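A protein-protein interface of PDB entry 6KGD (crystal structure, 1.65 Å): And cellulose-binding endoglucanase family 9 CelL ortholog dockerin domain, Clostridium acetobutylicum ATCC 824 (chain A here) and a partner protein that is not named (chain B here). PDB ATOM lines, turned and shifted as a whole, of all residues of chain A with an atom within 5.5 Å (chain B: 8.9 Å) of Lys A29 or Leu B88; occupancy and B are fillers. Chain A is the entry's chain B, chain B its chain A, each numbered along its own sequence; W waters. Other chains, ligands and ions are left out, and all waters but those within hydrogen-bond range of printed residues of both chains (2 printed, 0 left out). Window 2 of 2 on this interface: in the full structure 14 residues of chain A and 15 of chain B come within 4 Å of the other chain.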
ATOM      1  N   VAL A  20      24.127  25.077 -21.451  1.00  0.00           N
ATOM      2  CA  VAL A  20      24.860  23.873 -21.829  1.00  0.00           C
ATOM      3  C   VAL A  20      26.146  23.758 -21.028  1.00  0.00           C
ATOM      4  O   VAL A  20      26.478  22.680 -20.522  1.00  0.00           O
ATOM      5  CB  VAL A  20      25.150  23.870 -23.335  1.00  0.00           C
ATOM      6  CG1 VAL A  20      26.063  22.724 -23.694  1.00  0.00           C
ATOM      7  CG2 VAL A  20      23.855  23.779 -24.101  1.00  0.00           C
ATOM      8  N   ARG A  23      25.432  22.674 -17.510  1.00  0.00           N
ATOM      9  CA  ARG A  23      25.115  21.253 -17.462  1.00  0.00           C
ATOM     10  C   ARG A  23      26.359  20.402 -17.664  1.00  0.00           C
ATOM     11  O   ARG A  23      26.508  19.357 -17.016  1.00  0.00           O
ATOM     12  CB  ARG A  23      24.040  20.899 -18.479  1.00  0.00           C
ATOM     13  CG  ARG A  23      22.677  21.432 -18.097  1.00  0.00           C
ATOM     14  CD  ARG A  23      21.591  20.580 -18.707  1.00  0.00           C
ATOM     15  NE  ARG A  23      20.260  21.126 -18.477  1.00  0.00           N
ATOM     16  CZ  ARG A  23      19.521  21.713 -19.407  1.00  0.00           C
ATOM     17  NH1 ARG A  23      19.973  21.847 -20.633  1.00  0.00           N
ATOM     18  NH2 ARG A  23      18.317  22.165 -19.101  1.00  0.00           N
ATOM     19  N   GLN A  24      27.268  20.829 -18.549  1.00  0.00           N
ATOM     20  CA  GLN A  24      28.500  20.069 -18.747  1.00  0.00           C
ATOM     21  C   GLN A  24      29.325  20.043 -17.462  1.00  0.00           C
ATOM     22  O   GLN A  24      29.811  18.988 -17.053  1.00  0.00           O
ATOM     23  CB  GLN A  24      29.308  20.648 -19.902  1.00  0.00           C
ATOM     24  CG  GLN A  24      28.668  20.401 -21.273  1.00  0.00           C
ATOM     25  CD  GLN A  24      29.366  21.189 -22.347  1.00  0.00           C
ATOM     26  OE1 GLN A  24      29.842  22.300 -22.099  1.00  0.00           O
ATOM     27  NE2 GLN A  24      29.477  20.609 -23.536  1.00  0.00           N
ATOM     28  N   TYR A  25      29.451  21.194 -16.800  1.00  0.00           N
ATOM     29  CA  TYR A  25      30.191  21.266 -15.543  1.00  0.00           C
ATOM     30  C   TYR A  25      29.569  20.358 -14.487  1.00  0.00           C
ATOM     31  O   TYR A  25      30.274  19.626 -13.787  1.00  0.00           O
ATOM     32  CB  TYR A  25      30.244  22.729 -15.077  1.00  0.00           C
ATOM     33  CG  TYR A  25      31.082  22.974 -13.857  1.00  0.00           C
ATOM     34  CD1 TYR A  25      32.460  22.954 -13.924  1.00  0.00           C
ATOM     35  CD2 TYR A  25      30.478  23.198 -12.624  1.00  0.00           C
ATOM     36  CE1 TYR A  25      33.222  23.148 -12.787  1.00  0.00           C
ATOM     37  CE2 TYR A  25      31.236  23.417 -11.497  1.00  0.00           C
ATOM     38  CZ  TYR A  25      32.593  23.392 -11.586  1.00  0.00           C
ATOM     39  OH  TYR A  25      33.349  23.610 -10.457  1.00  0.00           O
ATOM     40  N   ALA A  27      27.885  17.728 -14.996  1.00  0.00           N
ATOM     41  CA  ALA A  27      28.019  16.341 -15.407  1.00  0.00           C
ATOM     42  C   ALA A  27      29.429  15.813 -15.261  1.00  0.00           C
ATOM     43  O   ALA A  27      29.690  14.667 -15.631  1.00  0.00           O
ATOM     44  CB  ALA A  27      27.569  16.186 -16.861  1.00  0.00           C
ATOM     45  N   GLY A  28      30.347  16.626 -14.759  1.00  0.00           N
ATOM     46  CA  GLY A  28      31.698  16.211 -14.497  1.00  0.00           C
ATOM     47  C   GLY A  28      32.688  16.525 -15.589  1.00  0.00           C
ATOM     48  O   GLY A  28      33.865  16.153 -15.463  1.00  0.00           O
ATOM     49  N   LYS A  29      32.268  17.199 -16.649  1.00  0.00           N
ATOM     50  CA  LYS A  29      33.173  17.455 -17.761  1.00  0.00           C
ATOM     51  C   LYS A  29      34.122  18.598 -17.419  1.00  0.00           C
ATOM     52  O   LYS A  29      33.807  19.478 -16.618  1.00  0.00           O
ATOM     53  CB  LYS A  29      32.378  17.772 -19.034  1.00  0.00           C
ATOM     54  CG  LYS A  29      31.762  16.557 -19.753  1.00  0.00           C
ATOM     55  CD  LYS A  29      30.289  16.303 -19.413  1.00  0.00           C
ATOM     56  CE  LYS A  29      29.573  15.566 -20.568  1.00  0.00           C
ATOM     57  NZ  LYS A  29      28.284  14.905 -20.177  1.00  0.00           N
ATOM     58  N   THR A  30      35.320  18.555 -18.001  1.00  0.00           N
ATOM     59  CA  THR A  30      36.204  19.714 -17.997  1.00  0.00           C
ATOM     60  C   THR A  30      35.772  20.615 -19.147  1.00  0.00           C
ATOM     61  O   THR A  30      35.796  20.195 -20.311  1.00  0.00           O
ATOM     62  CB  THR A  30      37.669  19.307 -18.152  1.00  0.00           C
ATOM     63  OG1 THR A  30      38.065  18.497 -17.039  1.00  0.00           O
ATOM     64  CG2 THR A  30      38.559  20.545 -18.201  1.00  0.00           C
ATOM     65  N   VAL A  31      35.364  21.837 -18.830  1.00  0.00           N
ATOM     66  CA  VAL A  31      34.717  22.718 -19.795  1.00  0.00           C
ATOM     67  C   VAL A  31      35.722  23.796 -20.162  1.00  0.00           C
ATOM     68  O   VAL A  31      36.098  24.612 -19.313  1.00  0.00           O
ATOM     69  CB  VAL A  31      33.426  23.325 -19.230  1.00  0.00           C
ATOM     70  CG1 VAL A  31      32.699  24.129 -20.298  1.00  0.00           C
ATOM     71  CG2 VAL A  31      32.517  22.230 -18.670  1.00  0.00           C
ATOM     72  N   GLY B  36      22.007  19.663 -30.484  1.00  0.00           N
ATOM     73  CA  GLY B  36      21.936  19.693 -29.039  1.00  0.00           C
ATOM     74  C   GLY B  36      21.526  21.019 -28.430  1.00  0.00           C
ATOM     75  O   GLY B  36      21.217  21.067 -27.228  1.00  0.00           O
ATOM     76  N   LEU B  37      21.529  22.093 -29.222  1.00  0.00           N
ATOM     77  CA  LEU B  37      21.194  23.430 -28.739  1.00  0.00           C
ATOM     78  C   LEU B  37      20.553  24.227 -29.864  1.00  0.00           C
ATOM     79  O   LEU B  37      21.098  24.276 -30.965  1.00  0.00           O
ATOM     80  CB  LEU B  37      22.435  24.159 -28.230  1.00  0.00           C
ATOM     81  CG  LEU B  37      22.296  25.636 -27.908  1.00  0.00           C
ATOM     82  CD1 LEU B  37      21.356  25.828 -26.723  1.00  0.00           C
ATOM     83  CD2 LEU B  37      23.630  26.276 -27.648  1.00  0.00           C
ATOM     84  N   ASP B  63      12.265  15.268 -22.477  1.00  0.00           N
ATOM     85  CA  ASP B  63      12.829  15.650 -21.179  1.00  0.00           C
ATOM     86  C   ASP B  63      12.435  17.068 -20.786  1.00  0.00           C
ATOM     87  O   ASP B  63      13.222  17.810 -20.186  1.00  0.00           O
ATOM     88  CB  ASP B  63      14.353  15.476 -21.199  1.00  0.00           C
ATOM     89  CG  ASP B  63      14.925  15.117 -19.851  1.00  0.00           C
ATOM     90  OD1 ASP B  63      14.161  14.678 -18.969  1.00  0.00           O
ATOM     91  OD2 ASP B  63      16.146  15.282 -19.661  1.00  0.00           O
ATOM     92  N   THR B  84      17.532  22.562 -25.377  1.00  0.00           N
ATOM     93  CA  THR B  84      18.758  21.880 -24.994  1.00  0.00           C
ATOM     94  C   THR B  84      18.414  20.430 -24.653  1.00  0.00           C
ATOM     95  O   THR B  84      17.267  20.103 -24.358  1.00  0.00           O
ATOM     96  CB  THR B  84      19.421  22.506 -23.762  1.00  0.00           C
ATOM     97  OG1 THR B  84      18.468  22.538 -22.676  1.00  0.00           O
ATOM     98  CG2 THR B  84      19.906  23.883 -24.031  1.00  0.00           C
ATOM     99  N   ASP B  85      19.420  19.557 -24.697  1.00  0.00           N
ATOM    100  CA  ASP B  85      19.243  18.185 -24.234  1.00  0.00           C
ATOM    101  C   ASP B  85      19.772  18.095 -22.816  1.00  0.00           C
ATOM    102  O   ASP B  85      20.994  18.113 -22.622  1.00  0.00           O
ATOM    103  CB  ASP B  85      19.965  17.200 -25.142  1.00  0.00           C
ATOM    104  CG  ASP B  85      19.931  15.761 -24.608  1.00  0.00           C
ATOM    105  OD1 ASP B  85      19.286  15.497 -23.569  1.00  0.00           O
ATOM    106  OD2 ASP B  85      20.558  14.906 -25.262  1.00  0.00           O
ATOM    107  N   PRO B  86      18.916  18.003 -21.800  1.00  0.00           N
ATOM    108  CA  PRO B  86      19.424  18.054 -20.420  1.00  0.00           C
ATOM    109  C   PRO B  86      20.348  16.911 -20.088  1.00  0.00           C
ATOM    110  O   PRO B  86      21.093  17.003 -19.100  1.00  0.00           O
ATOM    111  CB  PRO B  86      18.148  17.995 -19.568  1.00  0.00           C
ATOM    112  CG  PRO B  86      17.051  18.501 -20.475  1.00  0.00           C
ATOM    113  CD  PRO B  86      17.442  18.024 -21.853  1.00  0.00           C
ATOM    114  N   THR B  87      20.288  15.822 -20.854  1.00  0.00           N
ATOM    115  CA  THR B  87      21.111  14.644 -20.606  1.00  0.00           C
ATOM    116  C   THR B  87      22.451  14.684 -21.315  1.00  0.00           C
ATOM    117  O   THR B  87      23.312  13.827 -21.033  1.00  0.00           O
ATOM    118  CB  THR B  87      20.405  13.360 -21.053  1.00  0.00           C
ATOM    119  OG1 THR B  87      20.403  13.293 -22.478  1.00  0.00           O
ATOM    120  CG2 THR B  87      18.981  13.304 -20.537  1.00  0.00           C
ATOM    121  N   LEU B  88      22.657  15.644 -22.213  1.00  0.00           N
ATOM    122  CA  LEU B  88      23.892  15.797 -22.978  1.00  0.00           C
ATOM    123  C   LEU B  88      24.252  14.533 -23.751  1.00  0.00           C
ATOM    124  O   LEU B  88      25.422  14.278 -24.037  1.00  0.00           O
ATOM    125  CB  LEU B  88      25.055  16.216 -22.067  1.00  0.00           C
ATOM    126  CG  LEU B  88      24.782  17.520 -21.322  1.00  0.00           C
ATOM    127  CD1 LEU B  88      25.779  17.629 -20.166  1.00  0.00           C
ATOM    128  CD2 LEU B  88      24.843  18.741 -22.238  1.00  0.00           C
ATOM    129  N   ALA B  89      23.260  13.754 -24.146  1.00  0.00           N
ATOM    130  CA  ALA B  89      23.546  12.494 -24.806  1.00  0.00           C
ATOM    131  C   ALA B  89      22.326  11.858 -25.450  1.00  0.00           C
ATOM    132  O   ALA B  89      22.384  11.452 -26.619  1.00  0.00           O
ATOM    133  CB  ALA B  89      24.156  11.507 -23.797  1.00  0.00           C
ATOM    134  N   ASN B  90      21.229  11.753 -24.720  1.00  0.00           N
ATOM    135  CA  ASN B  90      20.177  10.831 -25.114  1.00  0.00           C
ATOM    136  C   ASN B  90      19.147  11.427 -26.059  1.00  0.00           C
ATOM    137  O   ASN B  90      18.501  10.671 -26.798  1.00  0.00           O
ATOM    138  CB  ASN B  90      19.402  10.317 -23.893  1.00  0.00           C
ATOM    139  CG  ASN B  90      20.289   9.595 -22.896  1.00  0.00           C
ATOM    140  OD1 ASN B  90      21.331   9.052 -23.253  1.00  0.00           O
ATOM    141  ND2 ASN B  90      19.871   9.590 -21.639  1.00  0.00           N
ATOM    142  N   TYR B  91      18.948  12.753 -26.037  1.00  0.00           N
ATOM    143  CA  TYR B  91      17.815  13.365 -26.728  1.00  0.00           C
ATOM    144  C   TYR B  91      18.182  14.567 -27.596  1.00  0.00           C
ATOM    145  O   TYR B  91      17.515  15.600 -27.545  1.00  0.00           O
ATOM    146  CB  TYR B  91      16.766  13.791 -25.706  1.00  0.00           C
ATOM    147  CG  TYR B  91      16.312  12.712 -24.761  1.00  0.00           C
ATOM    148  CD1 TYR B  91      15.858  11.488 -25.226  1.00  0.00           C
ATOM    149  CD2 TYR B  91      16.341  12.910 -23.389  1.00  0.00           C
ATOM    150  CE1 TYR B  91      15.438  10.503 -24.362  1.00  0.00           C
ATOM    151  CE2 TYR B  91      15.914  11.935 -22.524  1.00  0.00           C
ATOM    152  CZ  TYR B  91      15.469  10.731 -23.019  1.00  0.00           C
ATOM    153  OH  TYR B  91      15.042   9.748 -22.144  1.00  0.00           O
ATOM    154  N   PRO B  92      19.196  14.442 -28.450  1.00  0.00           N
ATOM    155  CA  PRO B  92      19.369  15.458 -29.483  1.00  0.00           C
ATOM    156  C   PRO B  92      18.222  15.374 -30.469  1.00  0.00           C
ATOM    157  O   PRO B  92      17.483  14.392 -30.541  1.00  0.00           O
ATOM    158  CB  PRO B  92      20.686  15.070 -30.160  1.00  0.00           C
ATOM    159  CG  PRO B  92      20.696  13.598 -30.041  1.00  0.00           C
ATOM    160  CD  PRO B  92      20.029  13.261 -28.709  1.00  0.00           C
ATOM    161  N   ASP B 128      25.749  21.419 -32.137  1.00  0.00           N
ATOM    162  CA  ASP B 128      25.632  19.970 -32.054  1.00  0.00           C
ATOM    163  C   ASP B 128      25.790  19.517 -30.610  1.00  0.00           C
ATOM    164  O   ASP B 128      25.802  20.325 -29.682  1.00  0.00           O
ATOM    165  CB  ASP B 128      26.609  19.291 -33.021  1.00  0.00           C
ATOM    166  CG  ASP B 128      28.063  19.458 -32.641  1.00  0.00           C
ATOM    167  OD1 ASP B 128      28.405  19.762 -31.472  1.00  0.00           O
ATOM    168  OD2 ASP B 128      28.891  19.254 -33.563  1.00  0.00           O
ATOM    169  N   GLU B 129      25.840  18.204 -30.392  1.00  0.00           N
ATOM    170  CA  GLU B 129      25.892  17.701 -29.026  1.00  0.00           C
ATOM    171  C   GLU B 129      27.210  18.016 -28.347  1.00  0.00           C
ATOM    172  O   GLU B 129      27.260  18.084 -27.114  1.00  0.00           O
ATOM    173  CB  GLU B 129      25.658  16.194 -29.006  1.00  0.00           C
ATOM    174  CG  GLU B 129      24.320  15.786 -29.571  1.00  0.00           C
ATOM    175  CD  GLU B 129      24.168  14.282 -29.669  1.00  0.00           C
ATOM    176  OE1 GLU B 129      23.767  13.656 -28.652  1.00  0.00           O
ATOM    177  OE2 GLU B 129      24.466  13.729 -30.757  1.00  0.00           O
ATOM    178  N   ASN B 130      28.273  18.219 -29.120  1.00  0.00           N
ATOM    179  CA  ASN B 130      29.581  18.554 -28.574  1.00  0.00           C
ATOM    180  C   ASN B 130      29.848  20.050 -28.626  1.00  0.00           C
ATOM    181  O   ASN B 130      31.002  20.477 -28.730  1.00  0.00           O
ATOM    182  CB  ASN B 130      30.655  17.761 -29.310  1.00  0.00           C
ATOM    183  CG  ASN B 130      30.540  16.267 -29.049  1.00  0.00           C
ATOM    184  OD1 ASN B 130      30.395  15.465 -29.972  1.00  0.00           O
ATOM    185  ND2 ASN B 130      30.574  15.891 -27.774  1.00  0.00           N
ATOM    186  N   ASP B 131      28.786  20.852 -28.559  1.00  0.00           N
ATOM    187  CA  ASP B 131      28.874  22.301 -28.408  1.00  0.00           C
ATOM    188  C   ASP B 131      29.534  22.976 -29.601  1.00  0.00           C
ATOM    189  O   ASP B 131      30.002  24.111 -29.488  1.00  0.00           O
ATOM    190  CB  ASP B 131      29.628  22.668 -27.122  1.00  0.00           C
ATOM    191  CG  ASP B 131      28.786  22.477 -25.878  1.00  0.00           C
ATOM    192  OD1 ASP B 131      28.117  21.425 -25.772  1.00  0.00           O
ATOM    193  OD2 ASP B 131      28.803  23.369 -25.000  1.00  0.00           O
HETATM  194  O   HOH W   1      27.782  13.453 -22.312  1.00  0.00           O
HETATM  195  O   HOH W   2      22.100  20.654 -22.228  1.00  0.00           O
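Thr B84 touches Val A20. Val A20 touches Asp B131 (CG1 to OD2, 3.1 Å). CD of Arg A23 touches O of Pro B86, 3.6 Å away. Arg A23 touches Leu B88 (O to CD1, 3.7 Å). Gln A24 touches Leu B88. Leu B88 touches Lys A29.
The backbone carbonyl oxygen of Gln A24 is in hydrogen-bond range of the backbone NH of Lys A29. The side-chain carboxylate of Asp B128 is in hydrogen-bond range of the backbone NH of Asp B131.
The side-chain hydroxyl of Thr B84 sits at hydrogen-bond distance from the guanidinium group of Arg A23, at 2.6 Å. The side-chain carboxylate of Asp B131 sits at hydrogen-bond distance from the side-chain amide nitrogen of Gln A24 (2.7 Å).
Printed residues of chain B within 4 Å of Val A20: Thr B84 (3.95 Å) and Asp B131 (3.1 Å). Of the printed residues of chain B, Arg A23 touches Thr B84 (2.6 Å), Pro B86 (3.6 Å) and Leu B88 (3.7 Å). No residue of chain B comes within 4 Å of Ala A27. Of chain B, only Leu B88 comes within 4 Å of Lys A29. Of the printed residues of chain A, Thr B84 touches Val A20 (3.95 Å) and Arg A23 (2.6 Å). Printed residues of chain A within 4 Å of Pro B86: Arg A23 (3.6 Å). Thr B87 touches none of the printed residues of chain A. Of the printed residues of chain A, Leu B88 touches Arg A23 (3.7 Å), Gln A24 (3.9 Å) and Lys A29 (3.7 Å). Asp B128 touches none of the printed residues of chain A. The nearest residue of chain B that does not touch Lys A29 is Thr B87 (5.2 Å).
Printed residues of chain A that touch a printed residue of chain B: Val A20, Arg A23, Gln A24 and Lys A29. Hydrophobic or aromatic side chains of chain A that line the printed part of chain B: Val A20. Of the 16 printed residues of chain B, 4 touch a printed residue of chain A. Hydrophobic or aromatic side chains of chain B that line the printed part of chain A: Pro B86 and Leu B88.
Water W1 bridges the side-chain amino group (NZ) of Lys A29 and the backbone carbonyl oxygen (O) of Leu B88. Water W2 lies within hydrogen-bond range of O of Asp B85 (2.8 Å) and NH1 of Arg A23 (2.9 Å).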
